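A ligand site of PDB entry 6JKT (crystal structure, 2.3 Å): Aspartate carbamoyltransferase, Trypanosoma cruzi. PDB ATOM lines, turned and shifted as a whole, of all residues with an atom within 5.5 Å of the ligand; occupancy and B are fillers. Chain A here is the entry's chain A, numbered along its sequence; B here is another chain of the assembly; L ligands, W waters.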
ATOM      1  N   ASP A  63      14.829  34.730 -11.455  1.00  0.00           N
ATOM      2  CA  ASP A  63      15.575  33.702 -10.725  1.00  0.00           C
ATOM      3  C   ASP A  63      15.077  32.266 -10.943  1.00  0.00           C
ATOM      4  O   ASP A  63      13.891  32.034 -11.153  1.00  0.00           O
ATOM      5  CB  ASP A  63      15.520  34.014  -9.238  1.00  0.00           C
ATOM      6  CG  ASP A  63      16.055  35.412  -8.908  1.00  0.00           C
ATOM      7  OD1 ASP A  63      17.110  35.791  -9.471  1.00  0.00           O
ATOM      8  OD2 ASP A  63      15.409  36.116  -8.121  1.00  0.00           O
ATOM      9  N   SER A  64      16.003  31.313 -10.891  1.00  0.00           N
ATOM     10  CA  SER A  64      15.685  29.905 -11.008  1.00  0.00           C
ATOM     11  C   SER A  64      16.795  29.092 -10.376  1.00  0.00           C
ATOM     12  O   SER A  64      17.965  29.492 -10.437  1.00  0.00           O
ATOM     13  CB  SER A  64      15.594  29.496 -12.480  1.00  0.00           C
ATOM     14  OG  SER A  64      15.315  28.096 -12.582  1.00  0.00           O
ATOM     15  N   SER A  65      16.424  27.987  -9.753  1.00  0.00           N
ATOM     16  CA  SER A  65      17.418  26.952  -9.413  1.00  0.00           C
ATOM     17  C   SER A  65      17.133  25.669 -10.168  1.00  0.00           C
ATOM     18  O   SER A  65      17.991  25.190 -10.912  1.00  0.00           O
ATOM     19  CB  SER A  65      17.445  26.668  -7.910  1.00  0.00           C
ATOM     20  OG  SER A  65      17.893  27.817  -7.230  1.00  0.00           O
ATOM     21  N   ARG A  66      15.946  25.134  -9.978  1.00  0.00           N
ATOM     22  CA  ARG A  66      15.527  23.902 -10.666  1.00  0.00           C
ATOM     23  C   ARG A  66      15.498  23.992 -12.180  1.00  0.00           C
ATOM     24  O   ARG A  66      16.103  23.177 -12.852  1.00  0.00           O
ATOM     25  CB  ARG A  66      14.158  23.435 -10.161  1.00  0.00           C
ATOM     26  CG  ARG A  66      14.233  22.550  -8.968  1.00  0.00           C
ATOM     27  CD  ARG A  66      13.053  22.853  -8.056  1.00  0.00           C
ATOM     28  NE  ARG A  66      13.223  24.200  -7.551  1.00  0.00           N
ATOM     29  CZ  ARG A  66      13.884  24.509  -6.438  1.00  0.00           C
ATOM     30  NH1 ARG A  66      14.420  23.545  -5.674  1.00  0.00           N
ATOM     31  NH2 ARG A  66      14.003  25.779  -6.110  1.00  0.00           N
ATOM     32  N   THR A  67      14.761  24.965 -12.710  1.00  0.00           N
ATOM     33  CA  THR A  67      14.522  24.965 -14.139  1.00  0.00           C
ATOM     34  C   THR A  67      15.836  25.175 -14.938  1.00  0.00           C
ATOM     35  O   THR A  67      16.159  24.393 -15.847  1.00  0.00           O
ATOM     36  CB  THR A  67      13.381  25.919 -14.532  1.00  0.00           C
ATOM     37  OG1 THR A  67      12.284  25.722 -13.599  1.00  0.00           O
ATOM     38  CG2 THR A  67      12.911  25.651 -15.969  1.00  0.00           C
ATOM     39  N   PHE A  68      16.592  26.200 -14.576  1.00  0.00           N
ATOM     40  CA  PHE A  68      17.929  26.438 -15.158  1.00  0.00           C
ATOM     41  C   PHE A  68      18.815  25.187 -15.051  1.00  0.00           C
ATOM     42  O   PHE A  68      19.335  24.683 -16.076  1.00  0.00           O
ATOM     43  CB  PHE A  68      18.606  27.623 -14.457  1.00  0.00           C
ATOM     44  CG  PHE A  68      20.026  27.848 -14.875  1.00  0.00           C
ATOM     45  CD1 PHE A  68      20.333  28.617 -15.997  1.00  0.00           C
ATOM     46  CD2 PHE A  68      21.069  27.276 -14.134  1.00  0.00           C
ATOM     47  CE1 PHE A  68      21.642  28.798 -16.380  1.00  0.00           C
ATOM     48  CE2 PHE A  68      22.391  27.460 -14.513  1.00  0.00           C
ATOM     49  CZ  PHE A  68      22.675  28.216 -15.649  1.00  0.00           C
ATOM     50  N   ARG A 115      12.919  32.159 -19.571  1.00  0.00           N
ATOM     51  CA  ARG A 115      12.060  32.507 -18.447  1.00  0.00           C
ATOM     52  C   ARG A 115      12.008  34.029 -18.348  1.00  0.00           C
ATOM     53  O   ARG A 115      13.066  34.667 -18.346  1.00  0.00           O
ATOM     54  CB  ARG A 115      12.615  31.928 -17.151  1.00  0.00           C
ATOM     55  CG  ARG A 115      11.883  32.444 -15.884  1.00  0.00           C
ATOM     56  CD  ARG A 115      12.294  31.660 -14.620  1.00  0.00           C
ATOM     57  NE  ARG A 115      11.664  30.335 -14.579  1.00  0.00           N
ATOM     58  CZ  ARG A 115      11.630  29.550 -13.506  1.00  0.00           C
ATOM     59  NH1 ARG A 115      12.209  29.921 -12.368  1.00  0.00           N
ATOM     60  NH2 ARG A 115      10.995  28.381 -13.585  1.00  0.00           N
ATOM     61  N   ALA A 136      10.175  28.486 -20.127  1.00  0.00           N
ATOM     62  CA  ALA A 136      10.572  28.002 -18.833  1.00  0.00           C
ATOM     63  C   ALA A 136       9.884  28.829 -17.743  1.00  0.00           C
ATOM     64  O   ALA A 136      10.307  28.806 -16.578  1.00  0.00           O
ATOM     65  CB  ALA A 136      12.087  28.053 -18.687  1.00  0.00           C
ATOM     66  N   HIS A 143       4.047  27.263 -17.284  1.00  0.00           N
ATOM     67  CA  HIS A 143       5.310  26.583 -17.156  1.00  0.00           C
ATOM     68  C   HIS A 143       5.173  25.224 -17.785  1.00  0.00           C
ATOM     69  O   HIS A 143       4.953  24.270 -17.077  1.00  0.00           O
ATOM     70  CB  HIS A 143       5.657  26.557 -15.669  1.00  0.00           C
ATOM     71  CG  HIS A 143       7.111  26.262 -15.322  1.00  0.00           C
ATOM     72  ND1 HIS A 143       7.948  25.623 -16.103  1.00  0.00           N
ATOM     73  CD2 HIS A 143       7.797  26.494 -14.187  1.00  0.00           C
ATOM     74  CE1 HIS A 143       9.103  25.502 -15.515  1.00  0.00           C
ATOM     75  NE2 HIS A 143       9.013  26.017 -14.348  1.00  0.00           N
ATOM     76  N   GLN A 146       7.239  22.078 -16.706  1.00  0.00           N
ATOM     77  CA  GLN A 146       6.933  21.685 -15.341  1.00  0.00           C
ATOM     78  C   GLN A 146       5.708  20.755 -15.327  1.00  0.00           C
ATOM     79  O   GLN A 146       5.733  19.713 -14.672  1.00  0.00           O
ATOM     80  CB  GLN A 146       6.708  22.908 -14.455  1.00  0.00           C
ATOM     81  CG  GLN A 146       6.504  22.583 -12.986  1.00  0.00           C
ATOM     82  CD  GLN A 146       7.811  22.269 -12.299  1.00  0.00           C
ATOM     83  OE1 GLN A 146       8.828  22.918 -12.552  1.00  0.00           O
ATOM     84  NE2 GLN A 146       7.786  21.272 -11.424  1.00  0.00           N
ATOM     85  N   ARG A 176       1.967  29.751 -12.092  1.00  0.00           N
ATOM     86  CA  ARG A 176       2.082  29.319 -13.483  1.00  0.00           C
ATOM     87  C   ARG A 176       2.199  27.793 -13.590  1.00  0.00           C
ATOM     88  O   ARG A 176       1.817  27.218 -14.600  1.00  0.00           O
ATOM     89  CB  ARG A 176       3.260  30.010 -14.187  1.00  0.00           C
ATOM     90  CG  ARG A 176       4.597  29.923 -13.485  1.00  0.00           C
ATOM     91  CD  ARG A 176       5.697  30.621 -14.297  1.00  0.00           C
ATOM     92  NE  ARG A 176       6.988  30.692 -13.601  1.00  0.00           N
ATOM     93  CZ  ARG A 176       7.883  31.659 -13.807  1.00  0.00           C
ATOM     94  NH1 ARG A 176       7.595  32.663 -14.648  1.00  0.00           N
ATOM     95  NH2 ARG A 176       9.047  31.640 -13.155  1.00  0.00           N
ATOM     96  N   THR A 177       2.719  27.149 -12.564  1.00  0.00           N
ATOM     97  CA  THR A 177       2.824  25.696 -12.552  1.00  0.00           C
ATOM     98  C   THR A 177       1.468  25.000 -12.525  1.00  0.00           C
ATOM     99  O   THR A 177       1.284  24.010 -13.241  1.00  0.00           O
ATOM    100  CB  THR A 177       3.624  25.202 -11.328  1.00  0.00           C
ATOM    101  OG1 THR A 177       2.961  25.651 -10.128  1.00  0.00           O
ATOM    102  CG2 THR A 177       5.053  25.769 -11.420  1.00  0.00           C
ATOM    103  N   ARG A 244       3.993  27.683  -3.538  1.00  0.00           N
ATOM    104  CA  ARG A 244       4.465  28.830  -2.776  1.00  0.00           C
ATOM    105  C   ARG A 244       3.644  30.085  -3.110  1.00  0.00           C
ATOM    106  O   ARG A 244       3.206  30.287  -4.232  1.00  0.00           O
ATOM    107  CB  ARG A 244       5.949  29.066  -3.084  1.00  0.00           C
ATOM    108  CG  ARG A 244       6.590  30.349  -2.489  1.00  0.00           C
ATOM    109  CD  ARG A 244       8.053  30.522  -2.976  1.00  0.00           C
ATOM    110  NE  ARG A 244       8.125  30.641  -4.424  1.00  0.00           N
ATOM    111  CZ  ARG A 244       8.154  31.814  -5.072  1.00  0.00           C
ATOM    112  NH1 ARG A 244       8.159  32.964  -4.398  1.00  0.00           N
ATOM    113  NH2 ARG A 244       8.206  31.829  -6.404  1.00  0.00           N
ATOM    114  N   GLN A 246       3.421  33.410  -4.479  1.00  0.00           N
ATOM    115  CA  GLN A 246       4.309  34.074  -5.385  1.00  0.00           C
ATOM    116  C   GLN A 246       4.386  35.556  -5.024  1.00  0.00           C
ATOM    117  O   GLN A 246       3.893  36.366  -5.729  1.00  0.00           O
ATOM    118  CB  GLN A 246       3.828  33.942  -6.809  1.00  0.00           C
ATOM    119  CG  GLN A 246       3.483  32.553  -7.223  1.00  0.00           C
ATOM    120  CD  GLN A 246       4.694  31.745  -7.561  1.00  0.00           C
ATOM    121  OE1 GLN A 246       5.362  32.007  -8.513  1.00  0.00           O
ATOM    122  NE2 GLN A 246       4.990  30.788  -6.773  1.00  0.00           N
ATOM    123  N   GLU A 248       6.587  37.913  -5.189  1.00  0.00           N
ATOM    124  CA  GLU A 248       7.188  38.819  -6.163  1.00  0.00           C
ATOM    125  C   GLU A 248       6.253  39.190  -7.300  1.00  0.00           C
ATOM    126  O   GLU A 248       6.560  40.080  -8.086  1.00  0.00           O
ATOM    127  CB  GLU A 248       8.509  38.245  -6.709  1.00  0.00           C
ATOM    128  CG  GLU A 248       8.395  36.989  -7.594  1.00  0.00           C
ATOM    129  CD  GLU A 248       8.229  35.669  -6.840  1.00  0.00           C
ATOM    130  OE1 GLU A 248       7.887  35.641  -5.632  1.00  0.00           O
ATOM    131  OE2 GLU A 248       8.431  34.614  -7.484  1.00  0.00           O
ATOM    132  N   ARG A 249       5.097  38.553  -7.373  1.00  0.00           N
ATOM    133  CA  ARG A 249       4.162  38.887  -8.448  1.00  0.00           C
ATOM    134  C   ARG A 249       3.001  39.773  -8.019  1.00  0.00           C
ATOM    135  O   ARG A 249       2.115  40.040  -8.824  1.00  0.00           O
ATOM    136  CB  ARG A 249       3.680  37.610  -9.146  1.00  0.00           C
ATOM    137  CG  ARG A 249       4.823  36.761  -9.588  1.00  0.00           C
ATOM    138  CD  ARG A 249       4.425  35.700 -10.545  1.00  0.00           C
ATOM    139  NE  ARG A 249       5.524  34.765 -10.751  1.00  0.00           N
ATOM    140  CZ  ARG A 249       6.558  34.971 -11.577  1.00  0.00           C
ATOM    141  NH1 ARG A 249       6.632  36.098 -12.283  1.00  0.00           N
ATOM    142  NH2 ARG A 249       7.511  34.049 -11.682  1.00  0.00           N
ATOM    143  N   HIS A 288       5.364  19.369  -4.943  1.00  0.00           N
ATOM    144  CA  HIS A 288       5.568  20.804  -4.867  1.00  0.00           C
ATOM    145  C   HIS A 288       6.650  21.072  -5.928  1.00  0.00           C
ATOM    146  O   HIS A 288       7.703  20.403  -5.907  1.00  0.00           O
ATOM    147  CB  HIS A 288       6.040  21.171  -3.449  1.00  0.00           C
ATOM    148  CG  HIS A 288       5.972  22.635  -3.122  1.00  0.00           C
ATOM    149  ND1 HIS A 288       6.509  23.604  -3.935  1.00  0.00           N
ATOM    150  CD2 HIS A 288       5.474  23.282  -2.029  1.00  0.00           C
ATOM    151  CE1 HIS A 288       6.319  24.792  -3.380  1.00  0.00           C
ATOM    152  NE2 HIS A 288       5.696  24.628  -2.229  1.00  0.00           N
ATOM    153  N   PRO A 289       6.391  22.017  -6.856  1.00  0.00           N
ATOM    154  CA  PRO A 289       7.378  22.292  -7.915  1.00  0.00           C
ATOM    155  C   PRO A 289       8.620  22.973  -7.338  1.00  0.00           C
ATOM    156  O   PRO A 289       9.674  23.012  -7.996  1.00  0.00           O
ATOM    157  CB  PRO A 289       6.645  23.310  -8.805  1.00  0.00           C
ATOM    158  CG  PRO A 289       5.726  24.044  -7.828  1.00  0.00           C
ATOM    159  CD  PRO A 289       5.254  22.955  -6.910  1.00  0.00           C
ATOM    160  N   LEU A 290       8.480  23.521  -6.116  1.00  0.00           N
ATOM    161  CA  LEU A 290       9.557  24.192  -5.372  1.00  0.00           C
ATOM    162  C   LEU A 290       9.964  25.562  -5.996  1.00  0.00           C
ATOM    163  O   LEU A 290       9.584  25.868  -7.147  1.00  0.00           O
ATOM    164  CB  LEU A 290      10.753  23.245  -5.137  1.00  0.00           C
ATOM    165  CG  LEU A 290      10.428  21.919  -4.404  1.00  0.00           C
ATOM    166  CD1 LEU A 290      11.660  21.030  -4.262  1.00  0.00           C
ATOM    167  CD2 LEU A 290       9.840  22.161  -3.034  1.00  0.00           C
ATOM    168  N   PRO A 291      10.660  26.443  -5.231  1.00  0.00           N
ATOM    169  CA  PRO A 291      11.051  26.316  -3.831  1.00  0.00           C
ATOM    170  C   PRO A 291       9.857  26.418  -2.887  1.00  0.00           C
ATOM    171  O   PRO A 291       8.830  27.009  -3.236  1.00  0.00           O
ATOM    172  CB  PRO A 291      11.985  27.503  -3.633  1.00  0.00           C
ATOM    173  CG  PRO A 291      11.482  28.521  -4.588  1.00  0.00           C
ATOM    174  CD  PRO A 291      10.993  27.768  -5.771  1.00  0.00           C
ATOM    175  N   SER B  91      16.992  30.387  -6.707  1.00  0.00           N
ATOM    176  CA  SER B  91      15.709  30.374  -6.027  1.00  0.00           C
ATOM    177  C   SER B  91      15.812  30.609  -4.507  1.00  0.00           C
ATOM    178  O   SER B  91      14.793  30.622  -3.806  1.00  0.00           O
ATOM    179  CB  SER B  91      14.885  29.135  -6.412  1.00  0.00           C
ATOM    180  OG  SER B  91      14.146  29.439  -7.588  1.00  0.00           O
ATOM    181  N   LYS B  94      13.790  33.374  -3.640  1.00  0.00           N
ATOM    182  CA  LYS B  94      12.381  33.036  -3.377  1.00  0.00           C
ATOM    183  C   LYS B  94      12.158  32.484  -1.956  1.00  0.00           C
ATOM    184  O   LYS B  94      11.052  32.084  -1.603  1.00  0.00           O
ATOM    185  CB  LYS B  94      11.859  32.025  -4.423  1.00  0.00           C
ATOM    186  CG  LYS B  94      11.749  32.523  -5.865  1.00  0.00           C
ATOM    187  CD  LYS B  94      11.591  31.320  -6.766  1.00  0.00           C
ATOM    188  CE  LYS B  94      11.514  31.713  -8.238  1.00  0.00           C
ATOM    189  NZ  LYS B  94      10.851  30.614  -9.094  1.00  0.00           N
ATOM    190  N   GLU B  96      14.188  29.897  -0.552  1.00  0.00           N
ATOM    191  CA  GLU B  96      14.751  28.527  -0.394  1.00  0.00           C
ATOM    192  C   GLU B  96      15.839  28.426   0.691  1.00  0.00           C
ATOM    193  O   GLU B  96      16.627  29.350   0.851  1.00  0.00           O
ATOM    194  CB  GLU B  96      15.305  28.007  -1.719  1.00  0.00           C
ATOM    195  CG  GLU B  96      15.481  26.508  -1.707  1.00  0.00           C
ATOM    196  CD  GLU B  96      15.332  25.897  -3.069  1.00  0.00           C
ATOM    197  OE1 GLU B  96      15.753  26.505  -4.069  1.00  0.00           O
ATOM    198  OE2 GLU B  96      14.773  24.777  -3.133  1.00  0.00           O
HETATM  199  P1  LIG L   1      12.842  27.185 -10.078  1.00  0.00           P
HETATM  200  O1  LIG L   1      13.846  26.747  -9.070  1.00  0.00           O
HETATM  201  O2  LIG L   1      13.243  26.982 -11.460  1.00  0.00           O
HETATM  202  O3  LIG L   1      12.259  28.537  -9.868  1.00  0.00           O
HETATM  203  C1  LIG L   1      11.492  26.083  -9.825  1.00  0.00           C
HETATM  204  C2  LIG L   1      10.195  26.631 -10.418  1.00  0.00           C
HETATM  205  O4  LIG L   1      10.060  26.702 -11.645  1.00  0.00           O
HETATM  206  N1  LIG L   1       9.271  26.993  -9.507  1.00  0.00           N
HETATM  207  C3  LIG L   1       7.943  27.497  -9.884  1.00  0.00           C
HETATM  208  C4  LIG L   1       8.033  28.773 -10.763  1.00  0.00           C
HETATM  209  O5  LIG L   1       9.112  29.397 -10.766  1.00  0.00           O
HETATM  210  O6  LIG L   1       7.023  29.086 -11.423  1.00  0.00           O
HETATM  211  C5  LIG L   1       7.109  27.750  -8.646  1.00  0.00           C
HETATM  212  C6  LIG L   1       7.680  28.822  -7.688  1.00  0.00           C
HETATM  213  O7  LIG L   1       7.311  28.732  -6.519  1.00  0.00           O
HETATM  214  O8  LIG L   1       8.474  29.688  -8.108  1.00  0.00           O
HETATM  215  O   HOH W   1       4.672  29.785 -10.083  1.00  0.00           O
HETATM  216  O   HOH W   2       5.350  27.036  -6.003  1.00  0.00           O
HETATM  217  O   HOH W   3       7.789  32.111  -9.770  1.00  0.00           O
HETATM  218  O   HOH W   4       3.698  27.777  -8.161  1.00  0.00           O
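An oxygen (O2) of the ligand lies within hydrogen-bond range of the side-chain hydroxyl (OG) of Ser 64, at 2.6 Å. An oxygen (O3) of the ligand lies within salt-bridge range of the side-chain amino group (NZ) of Lys 94 of chain B (2.6 Å). A nitrogen (N1) of the ligand sits at hydrogen-bond distance from the backbone carbonyl oxygen (O) of Leu 290. O2 of the ligand lies within hydrogen-bond range of N of Thr 67, at 2.8 Å. An oxygen (O2) of the ligand lies within hydrogen-bond range of the side-chain hydroxyl (OG1) of Thr 67 (2.7 Å). The guanidinium group (NE) of Arg 176 is in salt-bridge range of an oxygen (O6) of the ligand (2.7 Å). O3 of the ligand is in salt-bridge range of NH1 of Arg 115, at 2.9 Å. The guanidinium group (NH2) of Arg 244 lies within salt-bridge range of an oxygen (O8) of the ligand, at 2.7 Å. The backbone NH (N) of Arg 66 is in hydrogen-bond range of an oxygen (O1) of the ligand (2.8 Å). An oxygen (O1) of the ligand lies within salt-bridge range of the guanidinium group (NE) of Arg 66 (3.0 Å). The backbone NH (N) of Ser 65 lies within hydrogen-bond range of an oxygen (O1) of the ligand, at 2.9 Å. An oxygen (O4) of the ligand is in hydrogen-bond range of a ring nitrogen (NE2) of His 143, at 3.0 Å. OG of Ser 91 of chain B is in hydrogen-bond range of O1 of the ligand. The side-chain amide nitrogen (NE2) of Gln 246 sits at hydrogen-bond distance from an oxygen (O7) of the ligand (3.1 Å).
OG of Ser 64 sits at hydrogen-bond distance from N of Thr 67, 3.2 Å away. The backbone NH (N) of Phe 68 is in hydrogen-bond range of the side-chain hydroxyl (OG) of Ser 64 (3.0 Å). NH2 of Arg 115 lies within hydrogen-bond range of OG1 of Thr 67 (3.0 Å). The side-chain hydroxyl (OG1) of Thr 67 lies within hydrogen-bond range of a ring nitrogen (NE2) of His 143, at 3.4 Å. The guanidinium group of Arg 115 lies within hydrogen-bond range of a ring nitrogen (NE2) of His 143, at 3.2 Å. The guanidinium group (NE) of Arg 115 lies within hydrogen-bond range of the backbone carbonyl oxygen (O) of Ala 136 (2.9 Å). O of Arg 244 sits at hydrogen-bond distance from NE2 of Gln 246, at 3.1 Å. The backbone carbonyl oxygen (O) of Ser 91 of chain B lies close to the backbone NH (N) of Glu 96 of chain B (3.4 Å).
Water W2 lies within hydrogen-bond range of an oxygen (O7) of the ligand (2.6 Å) and the backbone NH of Arg 244 (2.9 Å). Water W1 lies within hydrogen-bond range of O6 of the ligand (2.8 Å), OE1 of Gln 246 (2.8 Å) and N of Arg 176 (3.4 Å).
CG2 of Thr 177 touches C3 of the ligand (3.7 Å). Pro 291 touches the ligand. Within 4 Å of the ligand: Ser 64, Ser 65, Arg 66, Thr 67, Arg 115, His 143, Arg 176, Thr 177, Arg 244, Gln 246, Leu 290, Pro 291, Ser 91 of chain B and Lys 94 of chain B. Along chain A the residues within 4 Å of the ligand span positions 64 to 291. The nearest printed residue that does not touch the ligand is Pro 289 (4.01 Å).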
